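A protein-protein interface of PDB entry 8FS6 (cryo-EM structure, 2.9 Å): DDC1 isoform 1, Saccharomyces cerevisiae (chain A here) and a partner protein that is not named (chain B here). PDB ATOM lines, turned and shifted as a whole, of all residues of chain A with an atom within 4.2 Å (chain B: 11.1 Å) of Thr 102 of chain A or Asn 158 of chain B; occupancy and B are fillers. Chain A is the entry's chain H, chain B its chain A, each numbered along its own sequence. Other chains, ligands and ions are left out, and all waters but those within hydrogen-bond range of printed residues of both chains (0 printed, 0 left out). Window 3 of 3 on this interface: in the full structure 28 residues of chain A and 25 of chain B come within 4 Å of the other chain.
The backbone carbonyl oxygen of Asn 158 of chain B sits close to the side-chain hydroxyl of Thr 25 of chain A, 2.4 Å away. OG of Ser 24 of chain A is in hydrogen-bond range of OD1 of Asn 158 of chain B (3.3 Å). The backbone carbonyl oxygen (O) of Ile 156 of chain B sits at hydrogen-bond distance from the guanidinium group (NE) of Arg 99 of chain A.
The backbone carbonyl oxygen of Tyr 21 of chain A lies within hydrogen-bond range of the side-chain hydroxyl of Ser 24 of chain A (2.6 Å).
Among the printed residues, pairs that only touch across the chains: Thr 25 of chain A with Val 157 of chain B (3.2 Å), Thr 102 of chain A with Asn 158 of chain B (3.3 Å), Arg 99 of chain A with Asn 158 of chain B (3.4 Å), Tyr 21 of chain A with Asp 159 of chain B (3.5 Å) and Thr 25 of chain A with Asp 159 of chain B (3.8 Å).
Of chain B, only Asp 159 comes within 4 Å of Tyr 21 of chain A. Of chain B, only Val 157 (3.2 Å), Asn 158 (2.4 Å) and Asp 159 (3.8 Å) come within 4 Å of Thr 25 of chain A. No residue of chain B comes within 4 Å of Gly 98 of chain A. No residue of chain B comes within 4 Å of Ile 104 of chain A. No residue of chain B comes within 4 Å of Ser 105 of chain A. Printed residues of chain A within 4 Å of Ile 156 of chain B: Arg 99 (3.4 Å). Printed residues of chain A within 4 Å of Val 157 of chain B: Thr 25 (3.2 Å). Asn 158 of chain B touches four residues of chain A. Printed residues of chain A within 4 Å of Asp 159 of chain B: Tyr 21 (3.5 Å) and Thr 25 (3.8 Å). The nearest residue of chain B that does not touch Thr 102 of chain A is Asp 159 of chain B (8.5 Å). The nearest printed residue of chain A that does not touch Asn 158 of chain B is Gly 98 of chain A (4.6 Å). The nearest printed residue of chain A that does not touch Val 157 of chain B is Ser 24 of chain A (4.3 Å).
Of the 13 printed residues of chain A, 5 touch a printed residue of chain B. Printed residues of chain A that touch a printed residue of chain B: Tyr 21, Ser 24, Thr 25, Arg 99 and Thr 102. Hydrophobic or aromatic side chains of chain A within 4 Å of the printed part of chain B: Tyr 21. Of the 13 printed residues of chain B, 4 touch a printed residue of chain A.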
ATOM      1  N   PHE A  17      30.659 -38.009  27.639  1.00  0.00           N
ATOM      2  CA  PHE A  17      30.562 -36.613  27.139  1.00  0.00           C
ATOM      3  C   PHE A  17      30.334 -36.586  25.624  1.00  0.00           C
ATOM      4  O   PHE A  17      29.443 -35.846  25.195  1.00  0.00           O
ATOM      5  CB  PHE A  17      31.818 -35.811  27.471  1.00  0.00           C
ATOM      6  CG  PHE A  17      31.896 -34.493  26.748  1.00  0.00           C
ATOM      7  CD1 PHE A  17      31.248 -33.373  27.241  1.00  0.00           C
ATOM      8  CD2 PHE A  17      32.596 -34.380  25.559  1.00  0.00           C
ATOM      9  CE1 PHE A  17      31.314 -32.164  26.569  1.00  0.00           C
ATOM     10  CE2 PHE A  17      32.660 -33.171  24.888  1.00  0.00           C
ATOM     11  CZ  PHE A  17      32.019 -32.065  25.395  1.00  0.00           C
ATOM     12  N   TYR A  21      27.122 -35.256  23.861  1.00  0.00           N
ATOM     13  CA  TYR A  21      27.367 -34.080  22.988  1.00  0.00           C
ATOM     14  C   TYR A  21      26.690 -34.318  21.648  1.00  0.00           C
ATOM     15  O   TYR A  21      26.165 -33.363  21.073  1.00  0.00           O
ATOM     16  CB  TYR A  21      28.854 -33.847  22.742  1.00  0.00           C
ATOM     17  CG  TYR A  21      29.125 -32.812  21.682  1.00  0.00           C
ATOM     18  CD1 TYR A  21      29.143 -33.153  20.341  1.00  0.00           C
ATOM     19  CD2 TYR A  21      29.320 -31.483  22.016  1.00  0.00           C
ATOM     20  CE1 TYR A  21      29.369 -32.204  19.359  1.00  0.00           C
ATOM     21  CE2 TYR A  21      29.550 -30.523  21.048  1.00  0.00           C
ATOM     22  CZ  TYR A  21      29.576 -30.884  19.714  1.00  0.00           C
ATOM     23  OH  TYR A  21      29.803 -29.942  18.754  1.00  0.00           O
ATOM     24  N   SER A  24      22.909 -34.199  21.962  1.00  0.00           N
ATOM     25  CA  SER A  24      22.492 -32.807  22.077  1.00  0.00           C
ATOM     26  C   SER A  24      22.513 -32.090  20.734  1.00  0.00           C
ATOM     27  O   SER A  24      21.696 -31.192  20.505  1.00  0.00           O
ATOM     28  CB  SER A  24      23.390 -32.071  23.072  1.00  0.00           C
ATOM     29  OG  SER A  24      24.664 -31.804  22.509  1.00  0.00           O
ATOM     30  N   THR A  25      23.438 -32.451  19.849  1.00  0.00           N
ATOM     31  CA  THR A  25      23.461 -31.864  18.516  1.00  0.00           C
ATOM     32  C   THR A  25      22.575 -32.609  17.527  1.00  0.00           C
ATOM     33  O   THR A  25      22.521 -32.225  16.355  1.00  0.00           O
ATOM     34  CB  THR A  25      24.890 -31.791  17.969  1.00  0.00           C
ATOM     35  OG1 THR A  25      24.883 -31.036  16.754  1.00  0.00           O
ATOM     36  CG2 THR A  25      25.428 -33.170  17.670  1.00  0.00           C
ATOM     37  N   GLY A  98      19.709 -30.958  26.190  1.00  0.00           N
ATOM     38  CA  GLY A  98      20.997 -31.456  25.734  1.00  0.00           C
ATOM     39  C   GLY A  98      22.131 -30.477  25.966  1.00  0.00           C
ATOM     40  O   GLY A  98      23.229 -30.871  26.369  1.00  0.00           O
ATOM     41  N   ARG A  99      21.887 -29.189  25.709  1.00  0.00           N
ATOM     42  CA  ARG A  99      22.927 -28.185  25.904  1.00  0.00           C
ATOM     43  C   ARG A  99      23.274 -28.027  27.379  1.00  0.00           C
ATOM     44  O   ARG A  99      24.442 -27.826  27.730  1.00  0.00           O
ATOM     45  CB  ARG A  99      22.484 -26.848  25.311  1.00  0.00           C
ATOM     46  CG  ARG A  99      22.331 -26.860  23.799  1.00  0.00           C
ATOM     47  CD  ARG A  99      21.839 -25.518  23.277  1.00  0.00           C
ATOM     48  NE  ARG A  99      20.455 -25.253  23.652  1.00  0.00           N
ATOM     49  CZ  ARG A  99      20.085 -24.436  24.628  1.00  0.00           C
ATOM     50  NH1 ARG A  99      20.974 -23.778  25.354  1.00  0.00           N
ATOM     51  NH2 ARG A  99      18.790 -24.274  24.882  1.00  0.00           N
ATOM     52  N   HIS A 100      22.271 -28.109  28.256  1.00  0.00           N
ATOM     53  CA  HIS A 100      22.532 -28.011  29.688  1.00  0.00           C
ATOM     54  C   HIS A 100      23.286 -29.233  30.197  1.00  0.00           C
ATOM     55  O   HIS A 100      24.112 -29.124  31.110  1.00  0.00           O
ATOM     56  CB  HIS A 100      21.218 -27.833  30.448  1.00  0.00           C
ATOM     57  CG  HIS A 100      20.582 -26.492  30.252  1.00  0.00           C
ATOM     58  ND1 HIS A 100      21.042 -25.578  29.328  1.00  0.00           N
ATOM     59  CD2 HIS A 100      19.522 -25.910  30.861  1.00  0.00           C
ATOM     60  CE1 HIS A 100      20.292 -24.491  29.377  1.00  0.00           C
ATOM     61  NE2 HIS A 100      19.363 -24.668  30.299  1.00  0.00           N
ATOM     62  N   LEU A 101      23.012 -30.407  29.625  1.00  0.00           N
ATOM     63  CA  LEU A 101      23.686 -31.620  30.076  1.00  0.00           C
ATOM     64  C   LEU A 101      25.114 -31.695  29.548  1.00  0.00           C
ATOM     65  O   LEU A 101      26.013 -32.180  30.244  1.00  0.00           O
ATOM     66  CB  LEU A 101      22.889 -32.852  29.649  1.00  0.00           C
ATOM     67  CG  LEU A 101      23.361 -34.194  30.209  1.00  0.00           C
ATOM     68  CD1 LEU A 101      23.523 -34.121  31.720  1.00  0.00           C
ATOM     69  CD2 LEU A 101      22.397 -35.305  29.825  1.00  0.00           C
ATOM     70  N   THR A 102      25.347 -31.216  28.322  1.00  0.00           N
ATOM     71  CA  THR A 102      26.677 -31.319  27.732  1.00  0.00           C
ATOM     72  C   THR A 102      27.663 -30.326  28.335  1.00  0.00           C
ATOM     73  O   THR A 102      28.876 -30.518  28.197  1.00  0.00           O
ATOM     74  CB  THR A 102      26.605 -31.130  26.213  1.00  0.00           C
ATOM     75  OG1 THR A 102      27.818 -31.602  25.614  1.00  0.00           O
ATOM     76  CG2 THR A 102      26.409 -29.665  25.855  1.00  0.00           C
ATOM     77  N   THR A 103      27.178 -29.277  28.999  1.00  0.00           N
ATOM     78  CA  THR A 103      28.053 -28.351  29.704  1.00  0.00           C
ATOM     79  C   THR A 103      28.365 -28.810  31.122  1.00  0.00           C
ATOM     80  O   THR A 103      29.169 -28.167  31.805  1.00  0.00           O
ATOM     81  CB  THR A 103      27.433 -26.948  29.736  1.00  0.00           C
ATOM     82  OG1 THR A 103      28.461 -25.973  29.951  1.00  0.00           O
ATOM     83  CG2 THR A 103      26.394 -26.837  30.841  1.00  0.00           C
ATOM     84  N   ILE A 104      27.751 -29.900  31.574  1.00  0.00           N
ATOM     85  CA  ILE A 104      28.060 -30.479  32.876  1.00  0.00           C
ATOM     86  C   ILE A 104      29.086 -31.599  32.751  1.00  0.00           C
ATOM     87  O   ILE A 104      30.022 -31.684  33.549  1.00  0.00           O
ATOM     88  CB  ILE A 104      26.763 -30.974  33.545  1.00  0.00           C
ATOM     89  CG1 ILE A 104      25.812 -29.805  33.800  1.00  0.00           C
ATOM     90  CG2 ILE A 104      27.068 -31.695  34.843  1.00  0.00           C
ATOM     91  CD1 ILE A 104      24.477 -30.221  34.376  1.00  0.00           C
ATOM     92  N   SER A 105      28.936 -32.455  31.741  1.00  0.00           N
ATOM     93  CA  SER A 105      29.819 -33.598  31.551  1.00  0.00           C
ATOM     94  C   SER A 105      31.114 -33.241  30.835  1.00  0.00           C
ATOM     95  O   SER A 105      31.951 -34.127  30.632  1.00  0.00           O
ATOM     96  CB  SER A 105      29.089 -34.697  30.773  1.00  0.00           C
ATOM     97  OG  SER A 105      28.652 -34.224  29.511  1.00  0.00           O
ATOM     98  N   ARG A 106      31.293 -31.983  30.439  1.00  0.00           N
ATOM     99  CA  ARG A 106      32.530 -31.568  29.793  1.00  0.00           C
ATOM    100  C   ARG A 106      33.702 -31.673  30.760  1.00  0.00           C
ATOM    101  O   ARG A 106      33.566 -31.406  31.959  1.00  0.00           O
ATOM    102  CB  ARG A 106      32.403 -30.137  29.273  1.00  0.00           C
ATOM    103  CG  ARG A 106      31.877 -29.156  30.307  1.00  0.00           C
ATOM    104  CD  ARG A 106      32.984 -28.264  30.846  1.00  0.00           C
ATOM    105  NE  ARG A 106      32.466 -26.994  31.341  1.00  0.00           N
ATOM    106  CZ  ARG A 106      31.907 -26.828  32.532  1.00  0.00           C
ATOM    107  NH1 ARG A 106      31.784 -27.834  33.384  1.00  0.00           N
ATOM    108  NH2 ARG A 106      31.459 -25.625  32.879  1.00  0.00           N
ATOM    109  N   ARG B 152       9.851 -26.514  13.874  1.00  0.00           N
ATOM    110  CA  ARG B 152       9.908 -25.890  15.189  1.00  0.00           C
ATOM    111  C   ARG B 152      11.052 -24.885  15.210  1.00  0.00           C
ATOM    112  O   ARG B 152      12.221 -25.267  15.093  1.00  0.00           O
ATOM    113  CB  ARG B 152      10.089 -26.942  16.283  1.00  0.00           C
ATOM    114  CG  ARG B 152       8.782 -27.540  16.781  1.00  0.00           C
ATOM    115  CD  ARG B 152       8.961 -28.361  18.054  1.00  0.00           C
ATOM    116  NE  ARG B 152      10.080 -27.907  18.872  1.00  0.00           N
ATOM    117  CZ  ARG B 152      11.214 -28.577  19.031  1.00  0.00           C
ATOM    118  NH1 ARG B 152      11.418 -29.741  18.436  1.00  0.00           N
ATOM    119  NH2 ARG B 152      12.166 -28.066  19.806  1.00  0.00           N
ATOM    120  N   ASP B 154      12.031 -22.894  17.753  1.00  0.00           N
ATOM    121  CA  ASP B 154      12.776 -22.918  19.013  1.00  0.00           C
ATOM    122  C   ASP B 154      13.414 -24.293  19.210  1.00  0.00           C
ATOM    123  O   ASP B 154      13.015 -25.097  20.055  1.00  0.00           O
ATOM    124  CB  ASP B 154      11.866 -22.543  20.176  1.00  0.00           C
ATOM    125  CG  ASP B 154      10.485 -23.158  20.058  1.00  0.00           C
ATOM    126  OD1 ASP B 154      10.115 -23.589  18.946  1.00  0.00           O
ATOM    127  OD2 ASP B 154       9.765 -23.207  21.078  1.00  0.00           O
ATOM    128  N   CYS B 155      14.439 -24.553  18.396  1.00  0.00           N
ATOM    129  CA  CYS B 155      15.213 -25.797  18.458  1.00  0.00           C
ATOM    130  C   CYS B 155      16.681 -25.419  18.268  1.00  0.00           C
ATOM    131  O   CYS B 155      17.164 -25.309  17.139  1.00  0.00           O
ATOM    132  CB  CYS B 155      14.742 -26.797  17.410  1.00  0.00           C
ATOM    133  SG  CYS B 155      15.648 -28.363  17.412  1.00  0.00           S
ATOM    134  N   ILE B 156      17.385 -25.227  19.383  1.00  0.00           N
ATOM    135  CA  ILE B 156      18.777 -24.774  19.356  1.00  0.00           C
ATOM    136  C   ILE B 156      19.652 -26.023  19.428  1.00  0.00           C
ATOM    137  O   ILE B 156      19.977 -26.526  20.504  1.00  0.00           O
ATOM    138  CB  ILE B 156      19.078 -23.783  20.477  1.00  0.00           C
ATOM    139  CG1 ILE B 156      18.032 -22.667  20.491  1.00  0.00           C
ATOM    140  CG2 ILE B 156      20.477 -23.207  20.314  1.00  0.00           C
ATOM    141  CD1 ILE B 156      18.331 -21.559  21.477  1.00  0.00           C
ATOM    142  N   VAL B 157      20.036 -26.528  18.256  1.00  0.00           N
ATOM    143  CA  VAL B 157      20.969 -27.646  18.183  1.00  0.00           C
ATOM    144  C   VAL B 157      22.377 -27.140  18.490  1.00  0.00           C
ATOM    145  O   VAL B 157      22.745 -26.010  18.143  1.00  0.00           O
ATOM    146  CB  VAL B 157      20.872 -28.313  16.796  1.00  0.00           C
ATOM    147  CG1 VAL B 157      22.142 -29.065  16.432  1.00  0.00           C
ATOM    148  CG2 VAL B 157      19.667 -29.245  16.745  1.00  0.00           C
ATOM    149  N   ASN B 158      23.161 -27.950  19.208  1.00  0.00           N
ATOM    150  CA  ASN B 158      24.583 -27.623  19.488  1.00  0.00           C
ATOM    151  C   ASN B 158      25.344 -27.825  18.183  1.00  0.00           C
ATOM    152  O   ASN B 158      25.065 -28.813  17.517  1.00  0.00           O
ATOM    153  CB  ASN B 158      25.194 -28.505  20.579  1.00  0.00           C
ATOM    154  CG  ASN B 158      25.279 -27.854  21.941  1.00  0.00           C
ATOM    155  OD1 ASN B 158      25.202 -28.540  22.957  1.00  0.00           O
ATOM    156  ND2 ASN B 158      25.460 -26.544  21.980  1.00  0.00           N
ATOM    157  N   ASP B 159      26.234 -26.910  17.811  1.00  0.00           N
ATOM    158  CA  ASP B 159      27.043 -27.035  16.575  1.00  0.00           C
ATOM    159  C   ASP B 159      26.173 -26.682  15.367  1.00  0.00           C
ATOM    160  O   ASP B 159      26.525 -27.111  14.252  1.00  0.00           O
ATOM    161  CB  ASP B 159      27.605 -28.448  16.428  1.00  0.00           C
ATOM    162  CG  ASP B 159      28.805 -28.554  15.504  1.00  0.00           C
ATOM    163  OD1 ASP B 159      29.365 -27.500  15.141  1.00  0.00           O
ATOM    164  OD2 ASP B 159      29.167 -29.694  15.149  1.00  0.00           O
ATOM    165  N   LEU B 160      25.072 -25.955  15.572  1.00  0.00           N
ATOM    166  CA  LEU B 160      24.178 -25.524  14.466  1.00  0.00           C
ATOM    167  C   LEU B 160      23.901 -24.026  14.591  1.00  0.00           C
ATOM    168  O   LEU B 160      23.032 -23.656  15.402  1.00  0.00           O
ATOM    169  CB  LEU B 160      22.867 -26.314  14.509  1.00  0.00           C
ATOM    170  CG  LEU B 160      21.906 -26.038  13.355  1.00  0.00           C
ATOM    171  CD1 LEU B 160      22.531 -26.422  12.024  1.00  0.00           C
ATOM    172  CD2 LEU B 160      20.593 -26.773  13.558  1.00  0.00           C
ATOM    173  N   PRO B 161      24.586 -23.148  13.830  1.00  0.00           N
ATOM    174  CA  PRO B 161      24.259 -21.720  13.837  1.00  0.00           C
ATOM    175  C   PRO B 161      22.781 -21.505  13.548  1.00  0.00           C
ATOM    176  O   PRO B 161      22.138 -22.294  12.852  1.00  0.00           O
ATOM    177  CB  PRO B 161      25.142 -21.143  12.723  1.00  0.00           C
ATOM    178  CG  PRO B 161      25.610 -22.317  11.925  1.00  0.00           C
ATOM    179  CD  PRO B 161      25.634 -23.481  12.853  1.00  0.00           C
ATOM    180  N   GLN B 162      22.239 -20.419  14.099  1.00  0.00           N
ATOM    181  CA  GLN B 162      20.803 -20.167  14.062  1.00  0.00           C
ATOM    182  C   GLN B 162      20.286 -19.766  12.683  1.00  0.00           C
ATOM    183  O   GLN B 162      19.106 -19.418  12.562  1.00  0.00           O
ATOM    184  CB  GLN B 162      20.432 -19.092  15.087  1.00  0.00           C
ATOM    185  CG  GLN B 162      19.786 -19.636  16.357  1.00  0.00           C
ATOM    186  CD  GLN B 162      18.480 -20.366  16.090  1.00  0.00           C
ATOM    187  OE1 GLN B 162      17.409 -19.761  16.092  1.00  0.00           O
ATOM    188  NE2 GLN B 162      18.561 -21.676  15.881  1.00  0.00           N
ATOM    189  N   GLU B 164      21.112 -21.967   9.963  1.00  0.00           N
ATOM    190  CA  GLU B 164      21.093 -23.234   9.248  1.00  0.00           C
ATOM    191  C   GLU B 164      20.050 -24.206   9.780  1.00  0.00           C
ATOM    192  O   GLU B 164      19.979 -25.340   9.294  1.00  0.00           O
ATOM    193  CB  GLU B 164      22.481 -23.885   9.303  1.00  0.00           C
ATOM    194  CG  GLU B 164      22.870 -24.644   8.043  1.00  0.00           C
ATOM    195  CD  GLU B 164      24.211 -25.339   8.176  1.00  0.00           C
ATOM    196  OE1 GLU B 164      24.760 -25.363   9.297  1.00  0.00           O
ATOM    197  OE2 GLU B 164      24.716 -25.859   7.159  1.00  0.00           O
ATOM    198  N   SER B 165      19.243 -23.800  10.763  1.00  0.00           N
ATOM    199  CA  SER B 165      18.224 -24.695  11.303  1.00  0.00           C
ATOM    200  C   SER B 165      17.185 -25.047  10.244  1.00  0.00           C
ATOM    201  O   SER B 165      16.833 -26.220  10.069  1.00  0.00           O
ATOM    202  CB  SER B 165      17.559 -24.057  12.523  1.00  0.00           C
ATOM    203  OG  SER B 165      16.873 -22.870  12.168  1.00  0.00           O
ATOM    204  N   GLU B 168      18.787 -27.356   7.586  1.00  0.00           N
ATOM    205  CA  GLU B 168      18.833 -28.744   8.040  1.00  0.00           C
ATOM    206  C   GLU B 168      17.444 -29.369   8.047  1.00  0.00           C
ATOM    207  O   GLU B 168      17.287 -30.549   7.714  1.00  0.00           O
ATOM    208  CB  GLU B 168      19.467 -28.824   9.428  1.00  0.00           C
ATOM    209  CG  GLU B 168      20.947 -28.479   9.452  1.00  0.00           C
ATOM    210  CD  GLU B 168      21.803 -29.537   8.783  1.00  0.00           C
ATOM    211  OE1 GLU B 168      22.478 -29.212   7.784  1.00  0.00           O
ATOM    212  OE2 GLU B 168      21.799 -30.692   9.255  1.00  0.00           O
